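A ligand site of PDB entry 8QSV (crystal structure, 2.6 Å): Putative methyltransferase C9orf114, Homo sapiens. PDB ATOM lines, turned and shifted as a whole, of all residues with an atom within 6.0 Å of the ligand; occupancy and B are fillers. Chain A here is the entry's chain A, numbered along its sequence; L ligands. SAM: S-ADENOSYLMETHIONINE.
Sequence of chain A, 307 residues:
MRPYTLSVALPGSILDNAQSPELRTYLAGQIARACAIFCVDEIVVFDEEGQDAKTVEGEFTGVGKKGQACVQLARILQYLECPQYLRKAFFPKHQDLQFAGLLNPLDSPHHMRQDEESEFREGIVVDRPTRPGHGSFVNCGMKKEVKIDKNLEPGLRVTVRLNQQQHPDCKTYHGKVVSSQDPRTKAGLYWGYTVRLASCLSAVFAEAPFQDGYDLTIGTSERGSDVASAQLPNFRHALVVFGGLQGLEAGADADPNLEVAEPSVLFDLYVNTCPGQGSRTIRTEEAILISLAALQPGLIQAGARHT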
ATOM      1  N   THR A 220     -32.259 -24.113  21.689  1.00  0.00           N
ATOM      2  CA  THR A 220     -30.899 -24.603  21.513  1.00  0.00           C
ATOM      3  C   THR A 220     -30.577 -24.937  20.072  1.00  0.00           C
ATOM      4  O   THR A 220     -31.362 -25.521  19.320  1.00  0.00           O
ATOM      5  CB  THR A 220     -30.685 -25.836  22.386  1.00  0.00           C
ATOM      6  OG1 THR A 220     -31.511 -26.890  21.882  1.00  0.00           O
ATOM      7  CG2 THR A 220     -30.965 -25.521  23.845  1.00  0.00           C
ATOM      8  N   SER A 221     -29.340 -24.561  19.697  1.00  0.00           N
ATOM      9  CA  SER A 221     -28.889 -24.694  18.327  1.00  0.00           C
ATOM     10  C   SER A 221     -27.422 -24.252  18.201  1.00  0.00           C
ATOM     11  O   SER A 221     -26.946 -23.371  18.913  1.00  0.00           O
ATOM     12  CB  SER A 221     -29.809 -23.941  17.379  1.00  0.00           C
ATOM     13  OG  SER A 221     -29.124 -23.500  16.221  1.00  0.00           O
ATOM     14  N   GLU A 222     -26.713 -24.924  17.290  1.00  0.00           N
ATOM     15  CA  GLU A 222     -25.380 -24.513  16.894  1.00  0.00           C
ATOM     16  C   GLU A 222     -25.365 -23.077  16.377  1.00  0.00           C
ATOM     17  O   GLU A 222     -24.334 -22.426  16.489  1.00  0.00           O
ATOM     18  CB  GLU A 222     -24.800 -25.491  15.865  1.00  0.00           C
ATOM     19  CG  GLU A 222     -25.626 -25.641  14.595  1.00  0.00           C
ATOM     20  CD  GLU A 222     -25.424 -26.962  13.879  1.00  0.00           C
ATOM     21  OE1 GLU A 222     -26.334 -27.827  13.961  1.00  0.00           O
ATOM     22  OE2 GLU A 222     -24.376 -27.126  13.234  1.00  0.00           O
ATOM     23  N   ARG A 223     -26.468 -22.562  15.815  1.00  0.00           N
ATOM     24  CA  ARG A 223     -26.413 -21.204  15.267  1.00  0.00           C
ATOM     25  C   ARG A 223     -27.089 -20.218  16.237  1.00  0.00           C
ATOM     26  O   ARG A 223     -27.417 -19.108  15.858  1.00  0.00           O
ATOM     27  CB  ARG A 223     -26.896 -21.128  13.803  1.00  0.00           C
ATOM     28  CG  ARG A 223     -28.212 -21.834  13.509  1.00  0.00           C
ATOM     29  CD  ARG A 223     -28.603 -21.761  12.040  1.00  0.00           C
ATOM     30  NE  ARG A 223     -28.112 -22.910  11.302  1.00  0.00           N
ATOM     31  CZ  ARG A 223     -28.648 -24.125  11.345  1.00  0.00           C
ATOM     32  NH1 ARG A 223     -29.898 -24.273  11.748  1.00  0.00           N
ATOM     33  NH2 ARG A 223     -27.955 -25.175  10.931  1.00  0.00           N
ATOM     34  N   VAL A 241     -35.794 -25.957  25.167  1.00  0.00           N
ATOM     35  CA  VAL A 241     -36.331 -26.682  24.035  1.00  0.00           C
ATOM     36  C   VAL A 241     -35.226 -27.205  23.131  1.00  0.00           C
ATOM     37  O   VAL A 241     -34.280 -26.486  22.834  1.00  0.00           O
ATOM     38  CB  VAL A 241     -37.279 -25.809  23.224  1.00  0.00           C
ATOM     39  CG1 VAL A 241     -37.951 -26.619  22.120  1.00  0.00           C
ATOM     40  CG2 VAL A 241     -38.296 -25.173  24.143  1.00  0.00           C
ATOM     41  N   PHE A 242     -35.405 -28.443  22.677  1.00  0.00           N
ATOM     42  CA  PHE A 242     -34.440 -29.102  21.822  1.00  0.00           C
ATOM     43  C   PHE A 242     -35.139 -29.540  20.568  1.00  0.00           C
ATOM     44  O   PHE A 242     -36.306 -29.921  20.631  1.00  0.00           O
ATOM     45  CB  PHE A 242     -33.831 -30.327  22.504  1.00  0.00           C
ATOM     46  CG  PHE A 242     -33.092 -29.972  23.770  1.00  0.00           C
ATOM     47  CD1 PHE A 242     -33.758 -29.909  24.997  1.00  0.00           C
ATOM     48  CD2 PHE A 242     -31.732 -29.675  23.750  1.00  0.00           C
ATOM     49  CE1 PHE A 242     -33.065 -29.613  26.165  1.00  0.00           C
ATOM     50  CE2 PHE A 242     -31.063 -29.339  24.918  1.00  0.00           C
ATOM     51  CZ  PHE A 242     -31.737 -29.286  26.120  1.00  0.00           C
ATOM     52  N   GLY A 243     -34.418 -29.508  19.452  1.00  0.00           N
ATOM     53  CA  GLY A 243     -34.926 -30.048  18.201  1.00  0.00           C
ATOM     54  C   GLY A 243     -34.506 -31.505  18.022  1.00  0.00           C
ATOM     55  O   GLY A 243     -33.689 -32.018  18.784  1.00  0.00           O
ATOM     56  N   GLY A 244     -35.100 -32.159  17.031  1.00  0.00           N
ATOM     57  CA  GLY A 244     -34.574 -33.411  16.518  1.00  0.00           C
ATOM     58  C   GLY A 244     -33.589 -33.138  15.393  1.00  0.00           C
ATOM     59  O   GLY A 244     -32.996 -32.060  15.345  1.00  0.00           O
ATOM     60  N   LEU A 245     -33.526 -34.080  14.449  1.00  0.00           N
ATOM     61  CA  LEU A 245     -32.480 -34.185  13.443  1.00  0.00           C
ATOM     62  C   LEU A 245     -32.414 -32.951  12.560  1.00  0.00           C
ATOM     63  O   LEU A 245     -31.339 -32.518  12.159  1.00  0.00           O
ATOM     64  CB  LEU A 245     -32.775 -35.452  12.617  1.00  0.00           C
ATOM     65  CG  LEU A 245     -31.752 -35.818  11.552  1.00  0.00           C
ATOM     66  CD1 LEU A 245     -30.341 -35.639  12.059  1.00  0.00           C
ATOM     67  CD2 LEU A 245     -31.942 -37.261  11.085  1.00  0.00           C
ATOM     68  N   GLN A 246     -33.567 -32.358  12.252  1.00  0.00           N
ATOM     69  CA  GLN A 246     -33.600 -31.232  11.347  1.00  0.00           C
ATOM     70  C   GLN A 246     -33.568 -29.914  12.126  1.00  0.00           C
ATOM     71  O   GLN A 246     -33.884 -28.865  11.584  1.00  0.00           O
ATOM     72  CB  GLN A 246     -34.834 -31.341  10.435  1.00  0.00           C
ATOM     73  CG  GLN A 246     -34.680 -32.332   9.300  1.00  0.00           C
ATOM     74  CD  GLN A 246     -33.294 -32.234   8.676  1.00  0.00           C
ATOM     75  OE1 GLN A 246     -32.869 -31.191   8.173  1.00  0.00           O
ATOM     76  NE2 GLN A 246     -32.555 -33.326   8.746  1.00  0.00           N
ATOM     77  N   GLY A 247     -33.188 -29.974  13.403  1.00  0.00           N
ATOM     78  CA  GLY A 247     -33.237 -28.787  14.256  1.00  0.00           C
ATOM     79  C   GLY A 247     -34.674 -28.373  14.564  1.00  0.00           C
ATOM     80  O   GLY A 247     -35.621 -29.055  14.169  1.00  0.00           O
ATOM     81  N   LEU A 248     -34.816 -27.256  15.301  1.00  0.00           N
ATOM     82  CA  LEU A 248     -36.107 -26.651  15.584  1.00  0.00           C
ATOM     83  C   LEU A 248     -36.709 -26.033  14.327  1.00  0.00           C
ATOM     84  O   LEU A 248     -37.892 -25.680  14.303  1.00  0.00           O
ATOM     85  CB  LEU A 248     -35.963 -25.570  16.670  1.00  0.00           C
ATOM     86  CG  LEU A 248     -35.697 -26.105  18.072  1.00  0.00           C
ATOM     87  CD1 LEU A 248     -35.374 -24.969  19.033  1.00  0.00           C
ATOM     88  CD2 LEU A 248     -36.871 -26.909  18.576  1.00  0.00           C
ATOM     89  N   GLU A 249     -35.902 -25.864  13.282  1.00  0.00           N
ATOM     90  CA  GLU A 249     -36.441 -25.289  12.062  1.00  0.00           C
ATOM     91  C   GLU A 249     -37.634 -26.123  11.637  1.00  0.00           C
ATOM     92  O   GLU A 249     -38.655 -25.559  11.251  1.00  0.00           O
ATOM     93  CB  GLU A 249     -35.381 -25.150  10.965  1.00  0.00           C
ATOM     94  CG  GLU A 249     -34.443 -23.966  11.178  1.00  0.00           C
ATOM     95  CD  GLU A 249     -33.358 -24.165  12.240  1.00  0.00           C
ATOM     96  OE1 GLU A 249     -33.267 -25.311  12.794  1.00  0.00           O
ATOM     97  OE2 GLU A 249     -32.588 -23.169  12.515  1.00  0.00           O
ATOM     98  N   VAL A 271     -29.466 -20.411  22.387  1.00  0.00           N
ATOM     99  CA  VAL A 271     -28.044 -20.595  22.706  1.00  0.00           C
ATOM    100  C   VAL A 271     -27.413 -21.769  21.957  1.00  0.00           C
ATOM    101  O   VAL A 271     -28.088 -22.766  21.644  1.00  0.00           O
ATOM    102  CB  VAL A 271     -27.852 -20.730  24.222  1.00  0.00           C
ATOM    103  CG1 VAL A 271     -28.114 -19.415  24.911  1.00  0.00           C
ATOM    104  CG2 VAL A 271     -28.761 -21.799  24.776  1.00  0.00           C
ATOM    105  N   ASN A 272     -26.123 -21.587  21.608  1.00  0.00           N
ATOM    106  CA  ASN A 272     -25.174 -22.662  21.321  1.00  0.00           C
ATOM    107  C   ASN A 272     -24.415 -22.978  22.601  1.00  0.00           C
ATOM    108  O   ASN A 272     -23.723 -22.126  23.145  1.00  0.00           O
ATOM    109  CB  ASN A 272     -24.176 -22.289  20.216  1.00  0.00           C
ATOM    110  CG  ASN A 272     -23.087 -23.319  19.994  1.00  0.00           C
ATOM    111  OD1 ASN A 272     -22.766 -24.119  20.880  1.00  0.00           O
ATOM    112  ND2 ASN A 272     -22.511 -23.349  18.806  1.00  0.00           N
ATOM    113  N   THR A 273     -24.552 -24.224  23.068  1.00  0.00           N
ATOM    114  CA  THR A 273     -24.051 -24.624  24.383  1.00  0.00           C
ATOM    115  C   THR A 273     -22.681 -25.291  24.304  1.00  0.00           C
ATOM    116  O   THR A 273     -22.026 -25.450  25.328  1.00  0.00           O
ATOM    117  CB  THR A 273     -25.080 -25.491  25.103  1.00  0.00           C
ATOM    118  OG1 THR A 273     -25.570 -26.514  24.229  1.00  0.00           O
ATOM    119  CG2 THR A 273     -26.251 -24.647  25.565  1.00  0.00           C
ATOM    120  N   CYS A 274     -22.217 -25.617  23.099  1.00  0.00           N
ATOM    121  CA  CYS A 274     -20.906 -26.224  22.945  1.00  0.00           C
ATOM    122  C   CYS A 274     -20.090 -25.445  21.931  1.00  0.00           C
ATOM    123  O   CYS A 274     -20.062 -25.759  20.732  1.00  0.00           O
ATOM    124  CB  CYS A 274     -21.091 -27.676  22.551  1.00  0.00           C
ATOM    125  SG  CYS A 274     -19.557 -28.618  22.676  1.00  0.00           S
ATOM    126  N   PRO A 275     -19.388 -24.372  22.340  1.00  0.00           N
ATOM    127  CA  PRO A 275     -18.594 -23.583  21.400  1.00  0.00           C
ATOM    128  C   PRO A 275     -17.500 -24.456  20.816  1.00  0.00           C
ATOM    129  O   PRO A 275     -16.972 -25.323  21.528  1.00  0.00           O
ATOM    130  CB  PRO A 275     -17.974 -22.457  22.256  1.00  0.00           C
ATOM    131  CG  PRO A 275     -18.131 -22.911  23.704  1.00  0.00           C
ATOM    132  CD  PRO A 275     -19.278 -23.894  23.724  1.00  0.00           C
ATOM    133  N   GLN A 277     -17.315 -27.033  18.638  1.00  0.00           N
ATOM    134  CA  GLN A 277     -17.585 -28.452  18.692  1.00  0.00           C
ATOM    135  C   GLN A 277     -16.776 -29.168  17.624  1.00  0.00           C
ATOM    136  O   GLN A 277     -16.671 -28.684  16.497  1.00  0.00           O
ATOM    137  CB  GLN A 277     -19.084 -28.685  18.519  1.00  0.00           C
ATOM    138  CG  GLN A 277     -19.581 -28.411  17.101  1.00  0.00           C
ATOM    139  CD  GLN A 277     -21.092 -28.443  17.020  1.00  0.00           C
ATOM    140  OE1 GLN A 277     -21.801 -27.607  17.584  1.00  0.00           O
ATOM    141  NE2 GLN A 277     -21.601 -29.420  16.292  1.00  0.00           N
ATOM    142  N   THR A 281     -22.129 -32.660  14.246  1.00  0.00           N
ATOM    143  CA  THR A 281     -23.432 -32.775  14.881  1.00  0.00           C
ATOM    144  C   THR A 281     -23.328 -33.225  16.324  1.00  0.00           C
ATOM    145  O   THR A 281     -22.414 -33.941  16.692  1.00  0.00           O
ATOM    146  CB  THR A 281     -24.354 -33.759  14.136  1.00  0.00           C
ATOM    147  OG1 THR A 281     -23.583 -34.928  13.878  1.00  0.00           O
ATOM    148  CG2 THR A 281     -24.951 -33.160  12.870  1.00  0.00           C
ATOM    149  N   ILE A 282     -24.269 -32.753  17.125  1.00  0.00           N
ATOM    150  CA  ILE A 282     -24.508 -33.191  18.482  1.00  0.00           C
ATOM    151  C   ILE A 282     -25.921 -33.723  18.515  1.00  0.00           C
ATOM    152  O   ILE A 282     -26.816 -32.999  18.170  1.00  0.00           O
ATOM    153  CB  ILE A 282     -24.382 -32.015  19.459  1.00  0.00           C
ATOM    154  CG1 ILE A 282     -22.990 -31.377  19.344  1.00  0.00           C
ATOM    155  CG2 ILE A 282     -24.698 -32.448  20.885  1.00  0.00           C
ATOM    156  CD1 ILE A 282     -22.863 -30.095  20.114  1.00  0.00           C
ATOM    157  N   ARG A 283     -26.110 -34.975  18.898  1.00  0.00           N
ATOM    158  CA  ARG A 283     -27.422 -35.586  18.890  1.00  0.00           C
ATOM    159  C   ARG A 283     -28.273 -34.991  20.010  1.00  0.00           C
ATOM    160  O   ARG A 283     -27.778 -34.414  20.959  1.00  0.00           O
ATOM    161  CB  ARG A 283     -27.278 -37.094  19.085  1.00  0.00           C
ATOM    162  CG  ARG A 283     -26.803 -37.917  17.887  1.00  0.00           C
ATOM    163  CD  ARG A 283     -27.029 -39.373  18.328  1.00  0.00           C
ATOM    164  NE  ARG A 283     -26.805 -40.397  17.333  1.00  0.00           N
ATOM    165  CZ  ARG A 283     -26.003 -41.463  17.515  1.00  0.00           C
ATOM    166  NH1 ARG A 283     -25.528 -41.741  18.713  1.00  0.00           N
ATOM    167  NH2 ARG A 283     -25.722 -42.288  16.513  1.00  0.00           N
ATOM    168  N   THR A 284     -29.590 -35.144  19.922  1.00  0.00           N
ATOM    169  CA  THR A 284     -30.467 -34.488  20.885  1.00  0.00           C
ATOM    170  C   THR A 284     -30.131 -34.952  22.308  1.00  0.00           C
ATOM    171  O   THR A 284     -29.925 -34.154  23.223  1.00  0.00           O
ATOM    172  CB  THR A 284     -31.926 -34.718  20.484  1.00  0.00           C
ATOM    173  OG1 THR A 284     -32.129 -34.220  19.156  1.00  0.00           O
ATOM    174  CG2 THR A 284     -32.914 -34.097  21.448  1.00  0.00           C
ATOM    175  N   ALA A 287     -27.059 -33.426  23.377  1.00  0.00           N
ATOM    176  CA  ALA A 287     -27.192 -31.986  23.504  1.00  0.00           C
ATOM    177  C   ALA A 287     -27.880 -31.608  24.822  1.00  0.00           C
ATOM    178  O   ALA A 287     -27.502 -30.610  25.425  1.00  0.00           O
ATOM    179  CB  ALA A 287     -27.936 -31.450  22.332  1.00  0.00           C
ATOM    180  N   SER A 291     -26.246 -29.113  27.281  1.00  0.00           N
ATOM    181  CA  SER A 291     -26.922 -27.836  27.452  1.00  0.00           C
ATOM    182  C   SER A 291     -27.312 -27.615  28.919  1.00  0.00           C
ATOM    183  O   SER A 291     -27.053 -26.549  29.493  1.00  0.00           O
ATOM    184  CB  SER A 291     -28.098 -27.788  26.524  1.00  0.00           C
ATOM    185  OG  SER A 291     -27.669 -28.015  25.182  1.00  0.00           O
HETATM  186  N   SAM L   1     -28.973 -30.023  11.348  1.00  0.00           N
HETATM  187  CA  SAM L   1     -29.661 -29.766  12.633  1.00  0.00           C
HETATM  188  C   SAM L   1     -29.714 -28.251  12.904  1.00  0.00           C
HETATM  189  O   SAM L   1     -29.622 -27.479  11.931  1.00  0.00           O
HETATM  190  OXT SAM L   1     -29.865 -27.890  14.076  1.00  0.00           O
HETATM  191  CB  SAM L   1     -28.950 -30.494  13.780  1.00  0.00           C
HETATM  192  CG  SAM L   1     -29.817 -30.707  15.002  1.00  0.00           C
HETATM  193  SD  SAM L   1     -28.972 -31.571  16.332  1.00  0.00           S
HETATM  194  CE  SAM L   1     -28.792 -33.186  15.587  1.00  0.00           C
HETATM  195  C5' SAM L   1     -30.341 -31.853  17.479  1.00  0.00           C
HETATM  196  C4' SAM L   1     -30.606 -30.748  18.495  1.00  0.00           C
HETATM  197  O4' SAM L   1     -29.558 -30.731  19.494  1.00  0.00           O
HETATM  198  C3' SAM L   1     -30.636 -29.318  17.970  1.00  0.00           C
HETATM  199  O3' SAM L   1     -31.866 -29.038  17.333  1.00  0.00           O
HETATM  200  C2' SAM L   1     -30.416 -28.565  19.285  1.00  0.00           C
HETATM  201  O2' SAM L   1     -31.583 -28.533  20.066  1.00  0.00           O
HETATM  202  C1' SAM L   1     -29.325 -29.412  19.931  1.00  0.00           C
HETATM  203  N9  SAM L   1     -27.970 -28.987  19.571  1.00  0.00           N
HETATM  204  C8  SAM L   1     -27.101 -29.507  18.638  1.00  0.00           C
HETATM  205  N7  SAM L   1     -25.965 -28.856  18.536  1.00  0.00           N
HETATM  206  C5  SAM L   1     -26.068 -27.861  19.488  1.00  0.00           C
HETATM  207  C6  SAM L   1     -25.191 -26.834  19.883  1.00  0.00           C
HETATM  208  N6  SAM L   1     -23.994 -26.624  19.340  1.00  0.00           N
HETATM  209  N1  SAM L   1     -25.609 -26.013  20.883  1.00  0.00           N
HETATM  210  C2  SAM L   1     -26.816 -26.217  21.420  1.00  0.00           C
HETATM  211  N3  SAM L   1     -27.735 -27.134  21.114  1.00  0.00           N
HETATM  212  C4  SAM L   1     -27.298 -27.934  20.132  1.00  0.00           C
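The backbone NH (N) of Ser 221 sits at hydrogen-bond distance from a nitrogen (N3) of the ligand.
O2' of the ligand is in hydrogen-bond range of O of Thr 220 (3.1 Å).
The backbone NH of Thr 273 lies within hydrogen-bond range of a nitrogen (N1) of the ligand (3.0 Å).
O of the ligand lies within salt-bridge range of NH2 of Arg 223 (3.0 Å).
The backbone NH (N) of Gly 243 sits at hydrogen-bond distance from an oxygen (O2') of the ligand (3.1 Å).
The side-chain amide oxygen of Asn 272 sits at hydrogen-bond distance from a nitrogen (N6) of the ligand (3.2 Å).
The side-chain amide oxygen (OE1) of Gln 277 sits at hydrogen-bond distance from a nitrogen (N6) of the ligand.
OG1 of Thr 220 is in hydrogen-bond range of O2' of the ligand, at 2.4 Å.
OG1 of Thr 273 lies close to N1 of the ligand, at 3.4 Å.
The backbone carbonyl oxygen of Ile 282 sits close to a sulfur (SD) of the ligand.
Residues that only touch the ligand: Leu 245 (3.3 Å), Ala 287 (3.3 Å), Gly 247 (3.4 Å), Phe 242 (3.4 Å), Thr 284 (3.4 Å), Gly 244 (3.4 Å), Glu 222 (3.5 Å), Val 271 (3.7 Å) and Gln 246 (3.9 Å).
Hydrophobic or aromatic side chains that line the ligand: Phe 242, Ile 282 and Ala 287.
17 residues have an atom within 4 Å of the ligand: Thr 220, Ser 221, Glu 222, Arg 223, Phe 242, Gly 243, Gly 244, Leu 245, Gln 246, Gly 247, Val 271, Asn 272, Thr 273, Gln 277, Ile 282, Thr 284 and Ala 287.
The nearest printed residue that does not touch the ligand is Leu 248 (4.001 Å).
N of Cys 274 lies within hydrogen-bond range of OD1 of Asn 272 (2.7 Å).
The backbone carbonyl oxygen (O) of Gly 243 is in hydrogen-bond range of the side-chain hydroxyl (OG1) of Thr 284, 2.7 Å away.
O of Val 271 lies within hydrogen-bond range of N of Ser 221, at 2.9 Å.
NH1 of Arg 223 is in salt-bridge range of OE2 of Glu 249.
The side-chain amide nitrogen of Asn 272 lies within hydrogen-bond range of the backbone carbonyl oxygen of Glu 222.
O of Ala 287 lies within hydrogen-bond range of OG of Ser 291 (2.6 Å).
The side-chain hydroxyl (OG1) of Thr 220 sits at hydrogen-bond distance from the backbone carbonyl oxygen (O) of Val 241 (3.0 Å).
N of Asn 272 sits close to O of Ser 221 (3.3 Å).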
